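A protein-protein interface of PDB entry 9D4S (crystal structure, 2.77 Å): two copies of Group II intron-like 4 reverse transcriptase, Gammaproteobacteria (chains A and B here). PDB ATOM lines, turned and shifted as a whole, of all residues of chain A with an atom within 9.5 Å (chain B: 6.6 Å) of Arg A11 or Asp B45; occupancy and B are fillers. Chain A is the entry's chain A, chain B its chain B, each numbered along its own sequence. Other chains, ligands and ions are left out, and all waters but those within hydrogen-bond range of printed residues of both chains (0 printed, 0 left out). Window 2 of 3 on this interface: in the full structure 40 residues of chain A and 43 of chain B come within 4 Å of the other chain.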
ATOM      1  N   LYS A   5      -4.039 -19.003  36.055  1.00  0.00           N
ATOM      2  CA  LYS A   5      -3.483 -19.565  34.822  1.00  0.00           C
ATOM      3  C   LYS A   5      -4.497 -19.443  33.705  1.00  0.00           C
ATOM      4  O   LYS A   5      -4.182 -19.084  32.568  1.00  0.00           O
ATOM      5  CB  LYS A   5      -3.146 -21.045  35.002  1.00  0.00           C
ATOM      6  CG  LYS A   5      -1.682 -21.359  35.258  1.00  0.00           C
ATOM      7  CD  LYS A   5      -1.509 -22.801  35.748  1.00  0.00           C
ATOM      8  CE  LYS A   5      -0.044 -23.158  36.032  1.00  0.00           C
ATOM      9  NZ  LYS A   5       0.082 -24.295  37.015  1.00  0.00           N
ATOM     10  N   ASP A   6      -5.738 -19.741  34.036  1.00  0.00           N
ATOM     11  CA  ASP A   6      -6.821 -19.625  33.093  1.00  0.00           C
ATOM     12  C   ASP A   6      -6.936 -18.222  32.532  1.00  0.00           C
ATOM     13  O   ASP A   6      -7.104 -18.045  31.324  1.00  0.00           O
ATOM     14  CB  ASP A   6      -8.093 -20.010  33.819  1.00  0.00           C
ATOM     15  CG  ASP A   6      -9.116 -20.450  32.913  1.00  0.00           C
ATOM     16  OD1 ASP A   6      -9.268 -19.793  31.845  1.00  0.00           O
ATOM     17  OD2 ASP A   6      -9.772 -21.498  33.184  1.00  0.00           O
ATOM     18  N   ILE A   7      -6.827 -17.214  33.388  1.00  0.00           N
ATOM     19  CA  ILE A   7      -7.017 -15.807  32.933  1.00  0.00           C
ATOM     20  C   ILE A   7      -5.862 -15.406  32.014  1.00  0.00           C
ATOM     21  O   ILE A   7      -6.070 -14.547  31.152  1.00  0.00           O
ATOM     22  CB  ILE A   7      -7.128 -14.872  34.153  1.00  0.00           C
ATOM     23  CG1 ILE A   7      -8.071 -15.438  35.215  1.00  0.00           C
ATOM     24  CG2 ILE A   7      -7.541 -13.472  33.727  1.00  0.00           C
ATOM     25  CD1 ILE A   7      -8.253 -14.542  36.411  1.00  0.00           C
ATOM     26  N   CYS A   8      -4.697 -16.021  32.188  1.00  0.00           N
ATOM     27  CA  CYS A   8      -3.500 -15.625  31.402  1.00  0.00           C
ATOM     28  C   CYS A   8      -3.398 -16.514  30.169  1.00  0.00           C
ATOM     29  O   CYS A   8      -2.360 -16.462  29.499  1.00  0.00           O
ATOM     30  CB  CYS A   8      -2.242 -15.746  32.253  1.00  0.00           C
ATOM     31  SG  CYS A   8      -2.296 -14.747  33.759  1.00  0.00           S
ATOM     32  N   SER A   9      -4.439 -17.297  29.896  1.00  0.00           N
ATOM     33  CA  SER A   9      -4.465 -18.156  28.688  1.00  0.00           C
ATOM     34  C   SER A   9      -4.739 -17.274  27.476  1.00  0.00           C
ATOM     35  O   SER A   9      -5.643 -16.440  27.557  1.00  0.00           O
ATOM     36  CB  SER A   9      -5.496 -19.231  28.806  1.00  0.00           C
ATOM     37  OG  SER A   9      -5.813 -19.772  27.537  1.00  0.00           O
ATOM     38  N   LEU A  10      -3.976 -17.469  26.402  1.00  0.00           N
ATOM     39  CA  LEU A  10      -4.155 -16.638  25.190  1.00  0.00           C
ATOM     40  C   LEU A  10      -5.458 -17.071  24.524  1.00  0.00           C
ATOM     41  O   LEU A  10      -6.007 -16.282  23.749  1.00  0.00           O
ATOM     42  CB  LEU A  10      -2.935 -16.793  24.282  1.00  0.00           C
ATOM     43  CG  LEU A  10      -2.628 -15.593  23.391  1.00  0.00           C
ATOM     44  CD1 LEU A  10      -2.169 -14.410  24.228  1.00  0.00           C
ATOM     45  CD2 LEU A  10      -1.573 -15.953  22.359  1.00  0.00           C
ATOM     46  N   ARG A  11      -5.938 -18.269  24.840  1.00  0.00           N
ATOM     47  CA  ARG A  11      -7.257 -18.692  24.316  1.00  0.00           C
ATOM     48  C   ARG A  11      -8.314 -17.965  25.139  1.00  0.00           C
ATOM     49  O   ARG A  11      -9.298 -17.503  24.544  1.00  0.00           O
ATOM     50  CB  ARG A  11      -7.411 -20.212  24.376  1.00  0.00           C
ATOM     51  CG  ARG A  11      -8.506 -20.741  23.462  1.00  0.00           C
ATOM     52  CD  ARG A  11      -9.043 -22.082  23.907  1.00  0.00           C
ATOM     53  NE  ARG A  11     -10.347 -22.347  23.324  1.00  0.00           N
ATOM     54  CZ  ARG A  11     -10.644 -23.419  22.603  1.00  0.00           C
ATOM     55  NH1 ARG A  11      -9.697 -24.281  22.281  1.00  0.00           N
ATOM     56  NH2 ARG A  11     -11.889 -23.625  22.210  1.00  0.00           N
ATOM     57  N   THR A  12      -8.120 -17.882  26.456  1.00  0.00           N
ATOM     58  CA  THR A  12      -9.051 -17.070  27.236  1.00  0.00           C
ATOM     59  C   THR A  12      -9.016 -15.625  26.771  1.00  0.00           C
ATOM     60  O   THR A  12     -10.063 -15.003  26.541  1.00  0.00           O
ATOM     61  CB  THR A  12      -8.721 -17.139  28.727  1.00  0.00           C
ATOM     62  OG1 THR A  12      -8.840 -18.485  29.187  1.00  0.00           O
ATOM     63  CG2 THR A  12      -9.675 -16.264  29.496  1.00  0.00           C
ATOM     64  N   LEU A  13      -7.817 -15.057  26.657  1.00  0.00           N
ATOM     65  CA  LEU A  13      -7.732 -13.661  26.280  1.00  0.00           C
ATOM     66  C   LEU A  13      -8.314 -13.439  24.899  1.00  0.00           C
ATOM     67  O   LEU A  13      -9.078 -12.489  24.691  1.00  0.00           O
ATOM     68  CB  LEU A  13      -6.281 -13.179  26.358  1.00  0.00           C
ATOM     69  CG  LEU A  13      -5.740 -13.211  27.792  1.00  0.00           C
ATOM     70  CD1 LEU A  13      -4.212 -13.270  27.807  1.00  0.00           C
ATOM     71  CD2 LEU A  13      -6.288 -12.037  28.630  1.00  0.00           C
ATOM     72  N   TYR A  14      -8.029 -14.342  23.953  1.00  0.00           N
ATOM     73  CA  TYR A  14      -8.532 -14.117  22.601  1.00  0.00           C
ATOM     74  C   TYR A  14     -10.041 -14.247  22.557  1.00  0.00           C
ATOM     75  O   TYR A  14     -10.712 -13.502  21.825  1.00  0.00           O
ATOM     76  CB  TYR A  14      -7.902 -15.073  21.572  1.00  0.00           C
ATOM     77  CG  TYR A  14      -8.307 -14.685  20.150  1.00  0.00           C
ATOM     78  CD1 TYR A  14      -7.619 -13.701  19.454  1.00  0.00           C
ATOM     79  CD2 TYR A  14      -9.412 -15.247  19.538  1.00  0.00           C
ATOM     80  CE1 TYR A  14      -8.013 -13.313  18.181  1.00  0.00           C
ATOM     81  CE2 TYR A  14      -9.808 -14.859  18.265  1.00  0.00           C
ATOM     82  CZ  TYR A  14      -9.105 -13.896  17.595  1.00  0.00           C
ATOM     83  OH  TYR A  14      -9.498 -13.511  16.326  1.00  0.00           O
ATOM     84  N   GLY A  15     -10.585 -15.190  23.332  1.00  0.00           N
ATOM     85  CA  GLY A  15     -12.027 -15.293  23.435  1.00  0.00           C
ATOM     86  C   GLY A  15     -12.643 -13.992  23.884  1.00  0.00           C
ATOM     87  O   GLY A  15     -13.581 -13.486  23.261  1.00  0.00           O
ATOM     88  N   ALA A  16     -12.075 -13.404  24.940  1.00  0.00           N
ATOM     89  CA  ALA A  16     -12.538 -12.105  25.395  1.00  0.00           C
ATOM     90  C   ALA A  16     -12.435 -11.076  24.277  1.00  0.00           C
ATOM     91  O   ALA A  16     -13.396 -10.346  24.008  1.00  0.00           O
ATOM     92  CB  ALA A  16     -11.741 -11.676  26.624  1.00  0.00           C
ATOM     93  N   TRP A  17     -11.290 -11.039  23.581  1.00  0.00           N
ATOM     94  CA  TRP A  17     -11.100 -10.041  22.528  1.00  0.00           C
ATOM     95  C   TRP A  17     -12.127 -10.211  21.423  1.00  0.00           C
ATOM     96  O   TRP A  17     -12.626  -9.221  20.875  1.00  0.00           O
ATOM     97  CB  TRP A  17      -9.686 -10.121  21.934  1.00  0.00           C
ATOM     98  CG  TRP A  17      -9.593  -9.420  20.608  1.00  0.00           C
ATOM     99  CD1 TRP A  17      -9.228  -9.962  19.418  1.00  0.00           C
ATOM    100  CD2 TRP A  17      -9.905  -8.039  20.343  1.00  0.00           C
ATOM    101  NE1 TRP A  17      -9.295  -9.012  18.417  1.00  0.00           N
ATOM    102  CE2 TRP A  17      -9.705  -7.824  18.962  1.00  0.00           C
ATOM    103  CE3 TRP A  17     -10.339  -6.971  21.137  1.00  0.00           C
ATOM    104  CZ2 TRP A  17      -9.918  -6.585  18.366  1.00  0.00           C
ATOM    105  CZ3 TRP A  17     -10.552  -5.735  20.533  1.00  0.00           C
ATOM    106  CH2 TRP A  17     -10.349  -5.558  19.166  1.00  0.00           C
ATOM    107  N   ARG A  18     -12.508 -11.447  21.128  1.00  0.00           N
ATOM    108  CA  ARG A  18     -13.472 -11.672  20.024  1.00  0.00           C
ATOM    109  C   ARG A  18     -14.785 -10.966  20.373  1.00  0.00           C
ATOM    110  O   ARG A  18     -15.332 -10.278  19.508  1.00  0.00           O
ATOM    111  CB  ARG A  18     -13.660 -13.167  19.757  1.00  0.00           C
ATOM    112  CG  ARG A  18     -14.502 -13.470  18.526  1.00  0.00           C
ATOM    113  CD  ARG A  18     -14.831 -14.938  18.366  1.00  0.00           C
ATOM    114  NE  ARG A  18     -15.764 -15.141  17.268  1.00  0.00           N
ATOM    115  CZ  ARG A  18     -16.247 -16.318  16.893  1.00  0.00           C
ATOM    116  NH1 ARG A  18     -16.005 -17.397  17.614  1.00  0.00           N
ATOM    117  NH2 ARG A  18     -16.962 -16.417  15.787  1.00  0.00           N
ATOM    118  N   LYS A  19     -15.267 -11.140  21.598  1.00  0.00           N
ATOM    119  CA  LYS A  19     -16.532 -10.496  22.030  1.00  0.00           C
ATOM    120  C   LYS A  19     -16.398  -8.969  22.015  1.00  0.00           C
ATOM    121  O   LYS A  19     -17.323  -8.308  21.528  1.00  0.00           O
ATOM    122  CB  LYS A  19     -16.881 -11.007  23.431  1.00  0.00           C
ATOM    123  CG  LYS A  19     -18.170 -10.470  24.036  1.00  0.00           C
ATOM    124  CD  LYS A  19     -19.409 -11.009  23.367  1.00  0.00           C
ATOM    125  CE  LYS A  19     -20.684 -10.415  23.930  1.00  0.00           C
ATOM    126  NZ  LYS A  19     -20.719  -8.947  23.759  1.00  0.00           N
ATOM    127  N   LEU A  47      -2.161  -8.878  22.164  1.00  0.00           N
ATOM    128  CA  LEU A  47      -2.651  -9.661  23.281  1.00  0.00           C
ATOM    129  C   LEU A  47      -1.537 -10.226  24.138  1.00  0.00           C
ATOM    130  O   LEU A  47      -1.710 -10.305  25.355  1.00  0.00           O
ATOM    131  CB  LEU A  47      -3.566 -10.785  22.774  1.00  0.00           C
ATOM    132  CG  LEU A  47      -5.079 -10.494  22.772  1.00  0.00           C
ATOM    133  CD1 LEU A  47      -5.875 -11.595  22.077  1.00  0.00           C
ATOM    134  CD2 LEU A  47      -5.622 -10.290  24.194  1.00  0.00           C
ATOM    135  N   GLN A  51      -0.985 -10.508  28.107  1.00  0.00           N
ATOM    136  CA  GLN A  51      -0.697 -11.805  28.761  1.00  0.00           C
ATOM    137  C   GLN A  51       0.556 -11.679  29.606  1.00  0.00           C
ATOM    138  O   GLN A  51       0.555 -12.165  30.742  1.00  0.00           O
ATOM    139  CB  GLN A  51      -0.430 -12.873  27.705  1.00  0.00           C
ATOM    140  CG  GLN A  51      -0.418 -14.289  28.255  1.00  0.00           C
ATOM    141  CD  GLN A  51       0.057 -15.274  27.220  1.00  0.00           C
ATOM    142  OE1 GLN A  51       0.533 -14.894  26.153  1.00  0.00           O
ATOM    143  NE2 GLN A  51      -0.050 -16.553  27.538  1.00  0.00           N
ATOM    144  N   VAL A  88     -10.845  -6.028  27.481  1.00  0.00           N
ATOM    145  CA  VAL A  88     -10.467  -7.416  27.235  1.00  0.00           C
ATOM    146  C   VAL A  88     -10.262  -8.137  28.556  1.00  0.00           C
ATOM    147  O   VAL A  88     -10.798  -9.233  28.773  1.00  0.00           O
ATOM    148  CB  VAL A  88      -9.216  -7.526  26.344  1.00  0.00           C
ATOM    149  CG1 VAL A  88      -8.850  -8.999  26.160  1.00  0.00           C
ATOM    150  CG2 VAL A  88      -9.437  -6.870  24.985  1.00  0.00           C
ATOM    151  N   ARG A  91     -13.648  -8.946  30.268  1.00  0.00           N
ATOM    152  CA  ARG A  91     -14.370 -10.086  29.719  1.00  0.00           C
ATOM    153  C   ARG A  91     -13.644 -11.391  30.019  1.00  0.00           C
ATOM    154  O   ARG A  91     -14.281 -12.422  30.264  1.00  0.00           O
ATOM    155  CB  ARG A  91     -14.561  -9.924  28.222  1.00  0.00           C
ATOM    156  CG  ARG A  91     -15.456 -10.997  27.616  1.00  0.00           C
ATOM    157  CD  ARG A  91     -16.798 -11.053  28.330  1.00  0.00           C
ATOM    158  NE  ARG A  91     -17.385 -12.386  28.275  1.00  0.00           N
ATOM    159  CZ  ARG A  91     -18.599 -12.634  27.809  1.00  0.00           C
ATOM    160  NH1 ARG A  91     -19.373 -11.661  27.360  1.00  0.00           N
ATOM    161  NH2 ARG A  91     -19.049 -13.885  27.796  1.00  0.00           N
ATOM    162  N   ALA A  92     -12.312 -11.369  29.989  1.00  0.00           N
ATOM    163  CA  ALA A  92     -11.533 -12.517  30.444  1.00  0.00           C
ATOM    164  C   ALA A  92     -11.936 -12.928  31.855  1.00  0.00           C
ATOM    165  O   ALA A  92     -12.145 -14.112  32.141  1.00  0.00           O
ATOM    166  CB  ALA A  92     -10.044 -12.181  30.396  1.00  0.00           C
ATOM    167  N   ASP A  95     -15.293 -14.594  31.853  1.00  0.00           N
ATOM    168  CA  ASP A  95     -15.340 -15.916  31.258  1.00  0.00           C
ATOM    169  C   ASP A  95     -14.762 -16.942  32.214  1.00  0.00           C
ATOM    170  O   ASP A  95     -15.328 -18.029  32.380  1.00  0.00           O
ATOM    171  CB  ASP A  95     -14.607 -15.905  29.923  1.00  0.00           C
ATOM    172  CG  ASP A  95     -15.347 -15.100  28.866  1.00  0.00           C
ATOM    173  OD1 ASP A  95     -16.579 -14.915  29.048  1.00  0.00           O
ATOM    174  OD2 ASP A  95     -14.712 -14.680  27.863  1.00  0.00           O
ATOM    175  N   VAL A  96     -13.677 -16.586  32.899  1.00  0.00           N
ATOM    176  CA  VAL A  96     -13.061 -17.503  33.852  1.00  0.00           C
ATOM    177  C   VAL A  96     -13.907 -17.628  35.117  1.00  0.00           C
ATOM    178  O   VAL A  96     -14.111 -18.731  35.645  1.00  0.00           O
ATOM    179  CB  VAL A  96     -11.631 -17.033  34.148  1.00  0.00           C
ATOM    180  CG1 VAL A  96     -10.956 -17.950  35.136  1.00  0.00           C
ATOM    181  CG2 VAL A  96     -10.831 -16.947  32.842  1.00  0.00           C
ATOM    182  N   ARG A  99     -16.798 -20.170  34.641  1.00  0.00           N
ATOM    183  CA  ARG A  99     -16.524 -21.574  34.246  1.00  0.00           C
ATOM    184  C   ARG A  99     -15.731 -22.289  35.333  1.00  0.00           C
ATOM    185  O   ARG A  99     -15.630 -23.516  35.257  1.00  0.00           O
ATOM    186  CB  ARG A  99     -15.661 -21.662  32.986  1.00  0.00           C
ATOM    187  CG  ARG A  99     -16.290 -21.074  31.734  1.00  0.00           C
ATOM    188  CD  ARG A  99     -15.217 -20.981  30.666  1.00  0.00           C
ATOM    189  NE  ARG A  99     -13.916 -20.785  31.290  1.00  0.00           N
ATOM    190  CZ  ARG A  99     -12.791 -20.560  30.626  1.00  0.00           C
ATOM    191  NH1 ARG A  99     -12.821 -19.935  29.466  1.00  0.00           N
ATOM    192  NH2 ARG A  99     -11.635 -20.944  31.139  1.00  0.00           N
ATOM    193  N   SER B  41     -13.057 -20.161  16.721  1.00  0.00           N
ATOM    194  CA  SER B  41     -13.056 -20.630  18.122  1.00  0.00           C
ATOM    195  C   SER B  41     -11.747 -21.395  18.247  1.00  0.00           C
ATOM    196  O   SER B  41     -11.264 -21.851  17.209  1.00  0.00           O
ATOM    197  CB  SER B  41     -14.219 -21.520  18.377  1.00  0.00           C
ATOM    198  OG  SER B  41     -15.398 -20.977  17.806  1.00  0.00           O
ATOM    199  N   ARG B  42     -11.174 -21.496  19.438  1.00  0.00           N
ATOM    200  CA  ARG B  42      -9.845 -22.143  19.568  1.00  0.00           C
ATOM    201  C   ARG B  42      -8.824 -21.377  18.742  1.00  0.00           C
ATOM    202  O   ARG B  42      -7.777 -21.962  18.459  1.00  0.00           O
ATOM    203  CB  ARG B  42      -9.840 -23.554  18.977  1.00  0.00           C
ATOM    204  CG  ARG B  42     -11.142 -24.336  19.053  1.00  0.00           C
ATOM    205  CD  ARG B  42     -11.061 -25.515  18.103  1.00  0.00           C
ATOM    206  NE  ARG B  42      -9.913 -26.351  18.421  1.00  0.00           N
ATOM    207  CZ  ARG B  42      -8.878 -26.551  17.615  1.00  0.00           C
ATOM    208  NH1 ARG B  42      -8.997 -26.354  16.317  1.00  0.00           N
ATOM    209  NH2 ARG B  42      -7.722 -26.945  18.118  1.00  0.00           N
ATOM    210  N   LEU B  43      -9.076 -20.108  18.425  1.00  0.00           N
ATOM    211  CA  LEU B  43      -8.169 -19.424  17.462  1.00  0.00           C
ATOM    212  C   LEU B  43      -6.714 -19.436  17.922  1.00  0.00           C
ATOM    213  O   LEU B  43      -5.869 -19.842  17.105  1.00  0.00           O
ATOM    214  CB  LEU B  43      -8.590 -17.995  17.111  1.00  0.00           C
ATOM    215  CG  LEU B  43      -7.804 -17.459  15.918  1.00  0.00           C
ATOM    216  CD1 LEU B  43      -7.883 -18.428  14.752  1.00  0.00           C
ATOM    217  CD2 LEU B  43      -8.282 -16.096  15.491  1.00  0.00           C
ATOM    218  N   PRO B  44      -6.338 -19.031  19.148  1.00  0.00           N
ATOM    219  CA  PRO B  44      -4.925 -19.023  19.461  1.00  0.00           C
ATOM    220  C   PRO B  44      -4.397 -20.415  19.105  1.00  0.00           C
ATOM    221  O   PRO B  44      -3.504 -20.494  18.313  1.00  0.00           O
ATOM    222  CB  PRO B  44      -4.914 -18.769  20.961  1.00  0.00           C
ATOM    223  CG  PRO B  44      -6.190 -18.005  21.207  1.00  0.00           C
ATOM    224  CD  PRO B  44      -7.198 -18.594  20.244  1.00  0.00           C
ATOM    225  N   ASP B  45      -5.047 -21.468  19.595  1.00  0.00           N
ATOM    226  CA  ASP B  45      -4.521 -22.851  19.443  1.00  0.00           C
ATOM    227  C   ASP B  45      -4.655 -23.371  18.009  1.00  0.00           C
ATOM    228  O   ASP B  45      -3.750 -24.084  17.576  1.00  0.00           O
ATOM    229  CB  ASP B  45      -5.204 -23.765  20.457  1.00  0.00           C
ATOM    230  CG  ASP B  45      -5.144 -23.224  21.875  1.00  0.00           C
ATOM    231  OD1 ASP B  45      -4.544 -22.154  22.069  1.00  0.00           O
ATOM    232  OD2 ASP B  45      -5.702 -23.877  22.774  1.00  0.00           O
ATOM    233  N   SER B  46      -5.751 -23.057  17.328  1.00  0.00           N
ATOM    234  CA  SER B  46      -5.942 -23.592  15.985  1.00  0.00           C
ATOM    235  C   SER B  46      -4.832 -23.125  15.030  1.00  0.00           C
ATOM    236  O   SER B  46      -4.454 -23.869  14.120  1.00  0.00           O
ATOM    237  CB  SER B  46      -7.352 -23.279  15.469  1.00  0.00           C
ATOM    238  OG  SER B  46      -7.709 -21.927  15.623  1.00  0.00           O
ATOM    239  N   LEU B  47      -4.270 -21.930  15.231  1.00  0.00           N
ATOM    240  CA  LEU B  47      -3.121 -21.523  14.427  1.00  0.00           C
ATOM    241  C   LEU B  47      -1.798 -22.036  15.002  1.00  0.00           C
ATOM    242  O   LEU B  47      -0.872 -22.312  14.238  1.00  0.00           O
ATOM    243  CB  LEU B  47      -3.056 -19.995  14.281  1.00  0.00           C
ATOM    244  CG  LEU B  47      -4.093 -19.210  13.454  1.00  0.00           C
ATOM    245  CD1 LEU B  47      -3.997 -17.721  13.734  1.00  0.00           C
ATOM    246  CD2 LEU B  47      -4.025 -19.456  11.952  1.00  0.00           C
ATOM    247  N   ILE B  48      -1.679 -22.173  16.328  1.00  0.00           N
ATOM    248  CA  ILE B  48      -0.459 -22.728  16.927  1.00  0.00           C
ATOM    249  C   ILE B  48      -0.227 -24.172  16.483  1.00  0.00           C
ATOM    250  O   ILE B  48       0.916 -24.633  16.379  1.00  0.00           O
ATOM    251  CB  ILE B  48      -0.520 -22.635  18.460  1.00  0.00           C
ATOM    252  CG1 ILE B  48      -0.805 -21.204  18.885  1.00  0.00           C
ATOM    253  CG2 ILE B  48       0.794 -23.079  19.057  1.00  0.00           C
ATOM    254  CD1 ILE B  48      -1.037 -21.044  20.354  1.00  0.00           C
ATOM    255  N   GLU B  49      -1.303 -24.933  16.306  1.00  0.00           N
ATOM    256  CA  GLU B  49      -1.179 -26.269  15.735  1.00  0.00           C
ATOM    257  C   GLU B  49      -0.431 -26.223  14.407  1.00  0.00           C
ATOM    258  O   GLU B  49       0.579 -26.914  14.209  1.00  0.00           O
ATOM    259  CB  GLU B  49      -2.566 -26.863  15.536  1.00  0.00           C
ATOM    260  CG  GLU B  49      -3.295 -27.234  16.791  1.00  0.00           C
ATOM    261  CD  GLU B  49      -4.777 -27.441  16.543  1.00  0.00           C
ATOM    262  OE1 GLU B  49      -5.219 -27.274  15.379  1.00  0.00           O
ATOM    263  OE2 GLU B  49      -5.502 -27.762  17.511  1.00  0.00           O
ATOM    264  N   ILE B  50      -0.936 -25.398  13.489  1.00  0.00           N
ATOM    265  CA  ILE B  50      -0.299 -25.185  12.195  1.00  0.00           C
ATOM    266  C   ILE B  50       1.132 -24.707  12.379  1.00  0.00           C
ATOM    267  O   ILE B  50       2.066 -25.248  11.777  1.00  0.00           O
ATOM    268  CB  ILE B  50      -1.136 -24.203  11.358  1.00  0.00           C
ATOM    269  CG1 ILE B  50      -2.541 -24.780  11.134  1.00  0.00           C
ATOM    270  CG2 ILE B  50      -0.415 -23.852  10.063  1.00  0.00           C
ATOM    271  CD1 ILE B  50      -3.661 -23.752  11.057  1.00  0.00           C
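Position printed for both chains: 47. Of the 7 pairs that touch across the chains among the printed residues, none has its exchanged pair printed and touching as well.
The side-chain hydroxyl of Ser A9 lies close to the backbone NH of Arg A11 (3.1 Å). O of Arg B42 is in hydrogen-bond range of OG of Ser B46 (2.8 Å). The guanidinium group of Arg B42 lies within salt-bridge range of the side-chain carboxylate of Glu B49 (2.4 Å). The backbone carbonyl oxygen (O) of Leu B43 lies close to the side-chain hydroxyl (OG) of Ser B46 (3.2 Å).
Hydrophobic or aromatic side chains of chain A that line the printed part of chain B: Tyr A14. Hydrophobic or aromatic side chains of chain B within 4 Å of the printed part of chain A: Leu B43 and Pro B44. Among the printed residues, no Asp or Glu carboxylate lies within 4 Å of a Lys or Arg side-chain nitrogen of the other chain.
Arg A11 touches three residues of chain B. Asp B45 touches one residue of chain A. No residue of chain A comes within 4 Å of Ser B46. Printed residues of chain B within 4 Å of Leu A10: Pro B44 (3.1 Å). Of the printed residues of chain A, Arg B42 touches Arg A11. Of the printed residues of chain A, Leu B43 touches Tyr A14 (3.0 Å). Of the printed residues of chain A, Ser B41 touches Arg A18. Of the printed residues of chain B, Tyr A14 touches Leu B43 and Pro B44.
Leu A10 touches Pro B44 (O to CG, 3.1 Å). Arg A11 touches Arg B42. Arg A11 touches Pro B44. Arg A11 touches Asp B45 (CD to OD2, 3.96 Å). CD2 of Leu B43 touches OH of Tyr A14, at 3.0 Å. CB of Tyr A14 touches CG of Pro B44, at 3.4 Å. OG of Ser B41 touches NH1 of Arg A18 (3.6 Å).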
